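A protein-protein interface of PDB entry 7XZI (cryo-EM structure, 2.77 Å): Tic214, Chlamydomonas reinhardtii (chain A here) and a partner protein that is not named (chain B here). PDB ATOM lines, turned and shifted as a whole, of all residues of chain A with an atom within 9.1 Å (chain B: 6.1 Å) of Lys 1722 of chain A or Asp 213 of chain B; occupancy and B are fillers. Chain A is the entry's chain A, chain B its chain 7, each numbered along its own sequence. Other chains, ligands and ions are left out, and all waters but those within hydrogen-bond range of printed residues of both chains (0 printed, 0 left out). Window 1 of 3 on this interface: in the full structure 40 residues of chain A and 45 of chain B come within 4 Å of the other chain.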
ATOM      1  N   ARG A1715      23.384 -15.491 -15.010  1.00  0.00           N
ATOM      2  CA  ARG A1715      23.030 -15.890 -16.369  1.00  0.00           C
ATOM      3  C   ARG A1715      22.052 -17.057 -16.371  1.00  0.00           C
ATOM      4  O   ARG A1715      21.132 -17.092 -17.197  1.00  0.00           O
ATOM      5  CB  ARG A1715      24.292 -16.245 -17.159  1.00  0.00           C
ATOM      6  CG  ARG A1715      24.024 -16.979 -18.462  1.00  0.00           C
ATOM      7  CD  ARG A1715      25.300 -17.184 -19.259  1.00  0.00           C
ATOM      8  NE  ARG A1715      25.800 -15.931 -19.805  1.00  0.00           N
ATOM      9  CZ  ARG A1715      25.376 -15.389 -20.941  1.00  0.00           C
ATOM     10  NH1 ARG A1715      24.440 -15.968 -21.675  1.00  0.00           N
ATOM     11  NH2 ARG A1715      25.901 -14.237 -21.346  1.00  0.00           N
ATOM     12  N   ARG A1716      22.237 -18.019 -15.466  1.00  0.00           N
ATOM     13  CA  ARG A1716      21.276 -19.110 -15.336  1.00  0.00           C
ATOM     14  C   ARG A1716      19.898 -18.583 -14.949  1.00  0.00           C
ATOM     15  O   ARG A1716      18.878 -19.017 -15.495  1.00  0.00           O
ATOM     16  CB  ARG A1716      21.773 -20.130 -14.309  1.00  0.00           C
ATOM     17  CG  ARG A1716      20.699 -21.057 -13.746  1.00  0.00           C
ATOM     18  CD  ARG A1716      20.076 -21.938 -14.818  1.00  0.00           C
ATOM     19  NE  ARG A1716      19.180 -22.938 -14.254  1.00  0.00           N
ATOM     20  CZ  ARG A1716      17.869 -22.777 -14.104  1.00  0.00           C
ATOM     21  NH1 ARG A1716      17.264 -21.659 -14.467  1.00  0.00           N
ATOM     22  NH2 ARG A1716      17.151 -23.764 -13.577  1.00  0.00           N
ATOM     23  N   LYS A1718      18.557 -15.410 -15.236  1.00  0.00           N
ATOM     24  CA  LYS A1718      17.892 -14.368 -16.009  1.00  0.00           C
ATOM     25  C   LYS A1718      17.823 -14.658 -17.502  1.00  0.00           C
ATOM     26  O   LYS A1718      16.971 -14.084 -18.192  1.00  0.00           O
ATOM     27  CB  LYS A1718      18.590 -13.026 -15.777  1.00  0.00           C
ATOM     28  CG  LYS A1718      18.763 -12.690 -14.305  1.00  0.00           C
ATOM     29  CD  LYS A1718      19.142 -11.238 -14.086  1.00  0.00           C
ATOM     30  CE  LYS A1718      19.510 -10.993 -12.632  1.00  0.00           C
ATOM     31  NZ  LYS A1718      18.506 -11.581 -11.703  1.00  0.00           N
ATOM     32  N   LYS A1719      18.682 -15.527 -18.026  1.00  0.00           N
ATOM     33  CA  LYS A1719      18.682 -15.825 -19.455  1.00  0.00           C
ATOM     34  C   LYS A1719      18.601 -17.332 -19.675  1.00  0.00           C
ATOM     35  O   LYS A1719      19.353 -17.915 -20.456  1.00  0.00           O
ATOM     36  CB  LYS A1719      19.905 -15.227 -20.146  1.00  0.00           C
ATOM     37  CG  LYS A1719      19.719 -15.044 -21.643  1.00  0.00           C
ATOM     38  CD  LYS A1719      20.929 -14.398 -22.288  1.00  0.00           C
ATOM     39  CE  LYS A1719      20.722 -14.241 -23.785  1.00  0.00           C
ATOM     40  NZ  LYS A1719      21.906 -13.633 -24.448  1.00  0.00           N
ATOM     41  N   ARG A1720      17.677 -17.978 -18.970  1.00  0.00           N
ATOM     42  CA  ARG A1720      17.419 -19.395 -19.193  1.00  0.00           C
ATOM     43  C   ARG A1720      16.886 -19.603 -20.603  1.00  0.00           C
ATOM     44  O   ARG A1720      15.773 -19.177 -20.925  1.00  0.00           O
ATOM     45  CB  ARG A1720      16.422 -19.914 -18.157  1.00  0.00           C
ATOM     46  CG  ARG A1720      16.153 -21.405 -18.232  1.00  0.00           C
ATOM     47  CD  ARG A1720      17.427 -22.207 -18.034  1.00  0.00           C
ATOM     48  NE  ARG A1720      17.145 -23.608 -17.755  1.00  0.00           N
ATOM     49  CZ  ARG A1720      18.076 -24.543 -17.596  1.00  0.00           C
ATOM     50  NH1 ARG A1720      19.363 -24.263 -17.703  1.00  0.00           N
ATOM     51  NH2 ARG A1720      17.700 -25.789 -17.324  1.00  0.00           N
ATOM     52  N   TYR A1721      17.686 -20.262 -21.446  1.00  0.00           N
ATOM     53  CA  TYR A1721      17.329 -20.393 -22.855  1.00  0.00           C
ATOM     54  C   TYR A1721      16.135 -21.315 -23.059  1.00  0.00           C
ATOM     55  O   TYR A1721      15.488 -21.262 -24.111  1.00  0.00           O
ATOM     56  CB  TYR A1721      18.530 -20.893 -23.657  1.00  0.00           C
ATOM     57  CG  TYR A1721      18.779 -20.111 -24.924  1.00  0.00           C
ATOM     58  CD1 TYR A1721      19.470 -18.908 -24.893  1.00  0.00           C
ATOM     59  CD2 TYR A1721      18.325 -20.573 -26.152  1.00  0.00           C
ATOM     60  CE1 TYR A1721      19.702 -18.188 -26.046  1.00  0.00           C
ATOM     61  CE2 TYR A1721      18.553 -19.859 -27.311  1.00  0.00           C
ATOM     62  CZ  TYR A1721      19.242 -18.666 -27.251  1.00  0.00           C
ATOM     63  OH  TYR A1721      19.474 -17.947 -28.400  1.00  0.00           O
ATOM     64  N   LYS A1722      15.837 -22.173 -22.082  1.00  0.00           N
ATOM     65  CA  LYS A1722      14.669 -23.042 -22.191  1.00  0.00           C
ATOM     66  C   LYS A1722      13.380 -22.228 -22.194  1.00  0.00           C
ATOM     67  O   LYS A1722      12.475 -22.478 -23.000  1.00  0.00           O
ATOM     68  CB  LYS A1722      14.663 -24.054 -21.044  1.00  0.00           C
ATOM     69  CG  LYS A1722      13.461 -24.982 -21.046  1.00  0.00           C
ATOM     70  CD  LYS A1722      13.373 -25.782 -19.755  1.00  0.00           C
ATOM     71  CE  LYS A1722      14.615 -26.631 -19.539  1.00  0.00           C
ATOM     72  NZ  LYS A1722      14.542 -27.392 -18.260  1.00  0.00           N
ATOM     73  N   LEU A1723      13.281 -21.243 -21.299  1.00  0.00           N
ATOM     74  CA  LEU A1723      12.044 -20.481 -21.169  1.00  0.00           C
ATOM     75  C   LEU A1723      11.846 -19.525 -22.340  1.00  0.00           C
ATOM     76  O   LEU A1723      10.742 -19.434 -22.890  1.00  0.00           O
ATOM     77  CB  LEU A1723      12.041 -19.719 -19.845  1.00  0.00           C
ATOM     78  CG  LEU A1723      12.280 -20.566 -18.594  1.00  0.00           C
ATOM     79  CD1 LEU A1723      12.180 -19.711 -17.343  1.00  0.00           C
ATOM     80  CD2 LEU A1723      11.298 -21.726 -18.536  1.00  0.00           C
ATOM     81  N   LEU A1724      12.895 -18.804 -22.735  1.00  0.00           N
ATOM     82  CA  LEU A1724      12.783 -17.823 -23.807  1.00  0.00           C
ATOM     83  C   LEU A1724      12.590 -18.460 -25.176  1.00  0.00           C
ATOM     84  O   LEU A1724      12.250 -17.751 -26.129  1.00  0.00           O
ATOM     85  CB  LEU A1724      14.016 -16.910 -23.818  1.00  0.00           C
ATOM     86  CG  LEU A1724      15.397 -17.497 -24.121  1.00  0.00           C
ATOM     87  CD1 LEU A1724      15.731 -17.410 -25.607  1.00  0.00           C
ATOM     88  CD2 LEU A1724      16.463 -16.796 -23.294  1.00  0.00           C
ATOM     89  N   LYS A1725      12.794 -19.771 -25.298  1.00  0.00           N
ATOM     90  CA  LYS A1725      12.539 -20.466 -26.550  1.00  0.00           C
ATOM     91  C   LYS A1725      11.053 -20.674 -26.802  1.00  0.00           C
ATOM     92  O   LYS A1725      10.624 -20.690 -27.962  1.00  0.00           O
ATOM     93  CB  LYS A1725      13.258 -21.818 -26.556  1.00  0.00           C
ATOM     94  CG  LYS A1725      13.284 -22.510 -27.910  1.00  0.00           C
ATOM     95  CD  LYS A1725      13.989 -23.853 -27.826  1.00  0.00           C
ATOM     96  CE  LYS A1725      15.403 -23.699 -27.295  1.00  0.00           C
ATOM     97  NZ  LYS A1725      16.222 -22.812 -28.164  1.00  0.00           N
ATOM     98  N   GLN A1726      10.259 -20.828 -25.740  1.00  0.00           N
ATOM     99  CA  GLN A1726       8.819 -21.028 -25.851  1.00  0.00           C
ATOM    100  C   GLN A1726       8.017 -19.922 -25.174  1.00  0.00           C
ATOM    101  O   GLN A1726       6.805 -20.078 -24.987  1.00  0.00           O
ATOM    102  CB  GLN A1726       8.430 -22.392 -25.270  1.00  0.00           C
ATOM    103  CG  GLN A1726       9.163 -22.768 -23.984  1.00  0.00           C
ATOM    104  CD  GLN A1726       8.388 -22.413 -22.728  1.00  0.00           C
ATOM    105  OE1 GLN A1726       7.428 -21.645 -22.770  1.00  0.00           O
ATOM    106  NE2 GLN A1726       8.799 -22.981 -21.601  1.00  0.00           N
ATOM    107  N   MET A1727       8.659 -18.810 -24.810  1.00  0.00           N
ATOM    108  CA  MET A1727       8.028 -17.701 -24.098  1.00  0.00           C
ATOM    109  C   MET A1727       6.778 -17.139 -24.778  1.00  0.00           C
ATOM    110  O   MET A1727       5.742 -17.015 -24.114  1.00  0.00           O
ATOM    111  CB  MET A1727       9.052 -16.579 -23.883  1.00  0.00           C
ATOM    112  CG  MET A1727       8.452 -15.247 -23.453  1.00  0.00           C
ATOM    113  SD  MET A1727       8.224 -14.102 -24.830  1.00  0.00           S
ATOM    114  CE  MET A1727       7.324 -12.779 -24.026  1.00  0.00           C
ATOM    115  N   PRO A1728       6.810 -16.782 -26.070  1.00  0.00           N
ATOM    116  CA  PRO A1728       5.658 -16.059 -26.640  1.00  0.00           C
ATOM    117  C   PRO A1728       4.346 -16.827 -26.593  1.00  0.00           C
ATOM    118  O   PRO A1728       3.287 -16.207 -26.441  1.00  0.00           O
ATOM    119  CB  PRO A1728       6.096 -15.788 -28.087  1.00  0.00           C
ATOM    120  CG  PRO A1728       7.102 -16.835 -28.378  1.00  0.00           C
ATOM    121  CD  PRO A1728       7.845 -17.027 -27.093  1.00  0.00           C
ATOM    122  N   ASN A1729       4.379 -18.155 -26.712  1.00  0.00           N
ATOM    123  CA  ASN A1729       3.135 -18.903 -26.874  1.00  0.00           C
ATOM    124  C   ASN A1729       2.507 -19.292 -25.537  1.00  0.00           C
ATOM    125  O   ASN A1729       1.278 -19.299 -25.413  1.00  0.00           O
ATOM    126  CB  ASN A1729       3.379 -20.144 -27.734  1.00  0.00           C
ATOM    127  CG  ASN A1729       4.494 -21.019 -27.199  1.00  0.00           C
ATOM    128  OD1 ASN A1729       4.251 -21.959 -26.444  1.00  0.00           O
ATOM    129  ND2 ASN A1729       5.726 -20.717 -27.594  1.00  0.00           N
ATOM    130  N   GLN A1730       3.322 -19.623 -24.529  1.00  0.00           N
ATOM    131  CA  GLN A1730       2.768 -20.170 -23.295  1.00  0.00           C
ATOM    132  C   GLN A1730       3.445 -19.631 -22.037  1.00  0.00           C
ATOM    133  O   GLN A1730       3.323 -20.246 -20.970  1.00  0.00           O
ATOM    134  CB  GLN A1730       2.866 -21.699 -23.302  1.00  0.00           C
ATOM    135  CG  GLN A1730       4.294 -22.217 -23.256  1.00  0.00           C
ATOM    136  CD  GLN A1730       4.409 -23.662 -23.691  1.00  0.00           C
ATOM    137  OE1 GLN A1730       4.660 -24.551 -22.876  1.00  0.00           O
ATOM    138  NE2 GLN A1730       4.235 -23.905 -24.984  1.00  0.00           N
ATOM    139  N   LEU A1731       4.145 -18.504 -22.122  1.00  0.00           N
ATOM    140  CA  LEU A1731       4.908 -18.011 -20.985  1.00  0.00           C
ATOM    141  C   LEU A1731       5.030 -16.497 -21.085  1.00  0.00           C
ATOM    142  O   LEU A1731       4.486 -15.864 -21.991  1.00  0.00           O
ATOM    143  CB  LEU A1731       6.290 -18.673 -20.922  1.00  0.00           C
ATOM    144  CG  LEU A1731       6.916 -18.887 -19.542  1.00  0.00           C
ATOM    145  CD1 LEU A1731       6.066 -19.834 -18.711  1.00  0.00           C
ATOM    146  CD2 LEU A1731       8.338 -19.411 -19.671  1.00  0.00           C
ATOM    147  N   TYR A1733       8.438 -13.941 -20.225  1.00  0.00           N
ATOM    148  CA  TYR A1733       9.822 -13.909 -19.761  1.00  0.00           C
ATOM    149  C   TYR A1733      10.517 -12.747 -20.453  1.00  0.00           C
ATOM    150  O   TYR A1733      10.918 -12.866 -21.615  1.00  0.00           O
ATOM    151  CB  TYR A1733      10.524 -15.232 -20.065  1.00  0.00           C
ATOM    152  CG  TYR A1733      11.781 -15.484 -19.269  1.00  0.00           C
ATOM    153  CD1 TYR A1733      11.713 -15.895 -17.947  1.00  0.00           C
ATOM    154  CD2 TYR A1733      13.035 -15.336 -19.846  1.00  0.00           C
ATOM    155  CE1 TYR A1733      12.855 -16.138 -17.216  1.00  0.00           C
ATOM    156  CE2 TYR A1733      14.184 -15.578 -19.123  1.00  0.00           C
ATOM    157  CZ  TYR A1733      14.087 -15.978 -17.808  1.00  0.00           C
ATOM    158  OH  TYR A1733      15.225 -16.221 -17.076  1.00  0.00           O
ATOM    159  N   GLU B 208      12.256 -23.698  -6.435  1.00  0.00           N
ATOM    160  CA  GLU B 208      12.158 -22.927  -7.669  1.00  0.00           C
ATOM    161  C   GLU B 208      12.979 -23.561  -8.784  1.00  0.00           C
ATOM    162  O   GLU B 208      12.528 -23.635  -9.933  1.00  0.00           O
ATOM    163  CB  GLU B 208      12.605 -21.483  -7.434  1.00  0.00           C
ATOM    164  CG  GLU B 208      11.536 -20.590  -6.831  1.00  0.00           C
ATOM    165  CD  GLU B 208      11.964 -19.138  -6.745  1.00  0.00           C
ATOM    166  OE1 GLU B 208      13.140 -18.844  -7.045  1.00  0.00           O
ATOM    167  OE2 GLU B 208      11.124 -18.290  -6.379  1.00  0.00           O
ATOM    168  N   TYR B 211      11.589 -27.325 -10.058  1.00  0.00           N
ATOM    169  CA  TYR B 211      10.272 -27.320 -10.690  1.00  0.00           C
ATOM    170  C   TYR B 211      10.032 -25.986 -11.384  1.00  0.00           C
ATOM    171  O   TYR B 211       9.034 -25.302 -11.153  1.00  0.00           O
ATOM    172  CB  TYR B 211       9.178 -27.610  -9.669  1.00  0.00           C
ATOM    173  CG  TYR B 211       9.356 -28.919  -8.934  1.00  0.00           C
ATOM    174  CD1 TYR B 211       9.704 -30.079  -9.613  1.00  0.00           C
ATOM    175  CD2 TYR B 211       9.187 -28.991  -7.558  1.00  0.00           C
ATOM    176  CE1 TYR B 211       9.872 -31.275  -8.942  1.00  0.00           C
ATOM    177  CE2 TYR B 211       9.354 -30.183  -6.881  1.00  0.00           C
ATOM    178  CZ  TYR B 211       9.696 -31.321  -7.576  1.00  0.00           C
ATOM    179  OH  TYR B 211       9.862 -32.509  -6.901  1.00  0.00           O
ATOM    180  N   GLU B 212      10.978 -25.595 -12.239  1.00  0.00           N
ATOM    181  CA  GLU B 212      10.937 -24.272 -12.854  1.00  0.00           C
ATOM    182  C   GLU B 212       9.751 -24.125 -13.802  1.00  0.00           C
ATOM    183  O   GLU B 212       9.058 -23.101 -13.789  1.00  0.00           O
ATOM    184  CB  GLU B 212      12.249 -24.008 -13.590  1.00  0.00           C
ATOM    185  CG  GLU B 212      12.345 -22.637 -14.230  1.00  0.00           C
ATOM    186  CD  GLU B 212      13.610 -22.476 -15.043  1.00  0.00           C
ATOM    187  OE1 GLU B 212      14.165 -23.503 -15.487  1.00  0.00           O
ATOM    188  OE2 GLU B 212      14.055 -21.325 -15.234  1.00  0.00           O
ATOM    189  N   ASP B 213       9.508 -25.134 -14.641  1.00  0.00           N
ATOM    190  CA  ASP B 213       8.536 -24.987 -15.720  1.00  0.00           C
ATOM    191  C   ASP B 213       7.125 -24.770 -15.180  1.00  0.00           C
ATOM    192  O   ASP B 213       6.449 -23.802 -15.543  1.00  0.00           O
ATOM    193  CB  ASP B 213       8.579 -26.214 -16.635  1.00  0.00           C
ATOM    194  CG  ASP B 213       9.917 -26.380 -17.328  1.00  0.00           C
ATOM    195  OD1 ASP B 213      10.612 -25.365 -17.542  1.00  0.00           O
ATOM    196  OD2 ASP B 213      10.270 -27.529 -17.666  1.00  0.00           O
ATOM    197  N   TYR B 214       6.669 -25.659 -14.296  1.00  0.00           N
ATOM    198  CA  TYR B 214       5.273 -25.628 -13.869  1.00  0.00           C
ATOM    199  C   TYR B 214       4.990 -24.440 -12.959  1.00  0.00           C
ATOM    200  O   TYR B 214       4.010 -23.715 -13.160  1.00  0.00           O
ATOM    201  CB  TYR B 214       4.911 -26.934 -13.165  1.00  0.00           C
ATOM    202  CG  TYR B 214       5.545 -28.153 -13.789  1.00  0.00           C
ATOM    203  CD1 TYR B 214       4.954 -28.791 -14.870  1.00  0.00           C
ATOM    204  CD2 TYR B 214       6.740 -28.662 -13.300  1.00  0.00           C
ATOM    205  CE1 TYR B 214       5.535 -29.905 -15.444  1.00  0.00           C
ATOM    206  CE2 TYR B 214       7.329 -29.772 -13.868  1.00  0.00           C
ATOM    207  CZ  TYR B 214       6.722 -30.391 -14.938  1.00  0.00           C
ATOM    208  OH  TYR B 214       7.308 -31.500 -15.504  1.00  0.00           O
ATOM    209  N   ILE B 215       5.843 -24.215 -11.964  1.00  0.00           N
ATOM    210  CA  ILE B 215       5.583 -23.265 -10.889  1.00  0.00           C
ATOM    211  C   ILE B 215       6.209 -21.927 -11.250  1.00  0.00           C
ATOM    212  O   ILE B 215       7.377 -21.869 -11.655  1.00  0.00           O
ATOM    213  CB  ILE B 215       6.124 -23.777  -9.545  1.00  0.00           C
ATOM    214  CG1 ILE B 215       5.535 -25.152  -9.227  1.00  0.00           C
ATOM    215  CG2 ILE B 215       5.814 -22.785  -8.432  1.00  0.00           C
ATOM    216  CD1 ILE B 215       6.093 -25.773  -7.969  1.00  0.00           C
ATOM    217  N   ALA B 216       5.429 -20.856 -11.110  1.00  0.00           N
ATOM    218  CA  ALA B 216       5.936 -19.510 -11.332  1.00  0.00           C
ATOM    219  C   ALA B 216       6.559 -18.900 -10.083  1.00  0.00           C
ATOM    220  O   ALA B 216       7.571 -18.198 -10.189  1.00  0.00           O
ATOM    221  CB  ALA B 216       4.817 -18.597 -11.842  1.00  0.00           C
ATOM    222  N   HIS B 241       2.230 -21.104 -13.503  1.00  0.00           N
ATOM    223  CA  HIS B 241       1.801 -20.411 -14.710  1.00  0.00           C
ATOM    224  C   HIS B 241       0.443 -20.937 -15.159  1.00  0.00           C
ATOM    225  O   HIS B 241       0.159 -22.133 -15.059  1.00  0.00           O
ATOM    226  CB  HIS B 241       2.826 -20.591 -15.830  1.00  0.00           C
ATOM    227  CG  HIS B 241       4.176 -20.032 -15.511  1.00  0.00           C
ATOM    228  ND1 HIS B 241       5.173 -20.781 -14.923  1.00  0.00           N
ATOM    229  CD2 HIS B 241       4.696 -18.796 -15.700  1.00  0.00           C
ATOM    230  CE1 HIS B 241       6.249 -20.031 -14.764  1.00  0.00           C
ATOM    231  NE2 HIS B 241       5.985 -18.821 -15.227  1.00  0.00           N
ATOM    232  N   ILE B 279      -0.478 -24.655 -16.905  1.00  0.00           N
ATOM    233  CA  ILE B 279       0.209 -25.071 -18.123  1.00  0.00           C
ATOM    234  C   ILE B 279       0.678 -26.517 -18.009  1.00  0.00           C
ATOM    235  O   ILE B 279       1.423 -27.006 -18.864  1.00  0.00           O
ATOM    236  CB  ILE B 279       1.396 -24.141 -18.433  1.00  0.00           C
ATOM    237  CG1 ILE B 279       2.519 -24.351 -17.415  1.00  0.00           C
ATOM    238  CG2 ILE B 279       0.951 -22.688 -18.426  1.00  0.00           C
ATOM    239  CD1 ILE B 279       3.780 -23.580 -17.734  1.00  0.00           C
ATOM    240  N   ASP B 283       1.804 -30.368 -20.916  1.00  0.00           N
ATOM    241  CA  ASP B 283       2.926 -31.243 -20.602  1.00  0.00           C
ATOM    242  C   ASP B 283       2.463 -32.660 -20.294  1.00  0.00           C
ATOM    243  O   ASP B 283       3.128 -33.621 -20.689  1.00  0.00           O
ATOM    244  CB  ASP B 283       3.727 -30.676 -19.428  1.00  0.00           C
ATOM    245  CG  ASP B 283       4.643 -29.539 -19.841  1.00  0.00           C
ATOM    246  OD1 ASP B 283       5.143 -29.562 -20.986  1.00  0.00           O
ATOM    247  OD2 ASP B 283       4.866 -28.624 -19.020  1.00  0.00           O
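The side-chain carboxylate (OE2) of Glu 212 of chain B lies within salt-bridge range of the guanidinium group (NH1) of Arg 1716 of chain A, 3.3 Å away. The side-chain carboxylate (OE1) of Glu 212 of chain B is in salt-bridge range of the guanidinium group (NE) of Arg 1720 of chain A.
O of Asp 213 of chain B lies within hydrogen-bond range of ND1 of His 241 of chain B (3.3 Å). The backbone carbonyl oxygen of Tyr 214 of chain B sits at hydrogen-bond distance from the backbone NH of His 241 of chain B. N of Ile 279 of chain B sits at hydrogen-bond distance from O of His 241 of chain B (3.2 Å).
Among the printed residues, merely in contact across the chains: Leu 1723 of chain A with Glu 212 of chain B (3.3 Å), Leu 1731 of chain A with His 241 of chain B (3.5 Å), Lys 1722 of chain A with Asp 213 of chain B (3.6 Å) and Leu 1723 of chain A with Asp 213 of chain B (3.8 Å).
Printed residues of chain B within 4 Å of Arg 1720 of chain A: Glu 212. Of chain B, only Asp 213 (3.6 Å) comes within 4 Å of Lys 1722 of chain A. Printed residues of chain B within 4 Å of Leu 1731 of chain A: His 241 (3.5 Å). Tyr 211 of chain B touches none of the printed residues of chain A. Of the printed residues of chain A, Glu 212 of chain B touches Arg 1716 (3.3 Å), Arg 1720 (3.7 Å) and Leu 1723 (3.3 Å). Of chain A, only Lys 1722 (3.6 Å) and Leu 1723 (3.8 Å) come within 4 Å of Asp 213 of chain B. The nearest residue of chain B that does not touch Lys 1722 of chain A is Glu 212 of chain B (4.8 Å). The nearest residue of chain A that does not touch Asp 213 of chain B is Gln 1726 of chain A (5.0 Å).
Of the 17 printed residues of chain A, 5 touch a printed residue of chain B. Hydrophobic or aromatic side chains of chain A that line the printed part of chain B: Leu 1723 and Leu 1731. Along chain A the printed residues that touch a printed residue of chain B span positions 1716 to 1731. Among the printed residues, Asp or Glu carboxylates within 4 Å of a Lys or Arg side-chain nitrogen of the other chain: Arg 1716 of chain A with Glu 212 of chain B (3.3 Å) and Arg 1720 of chain A with Glu 212 of chain B (3.7 Å).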
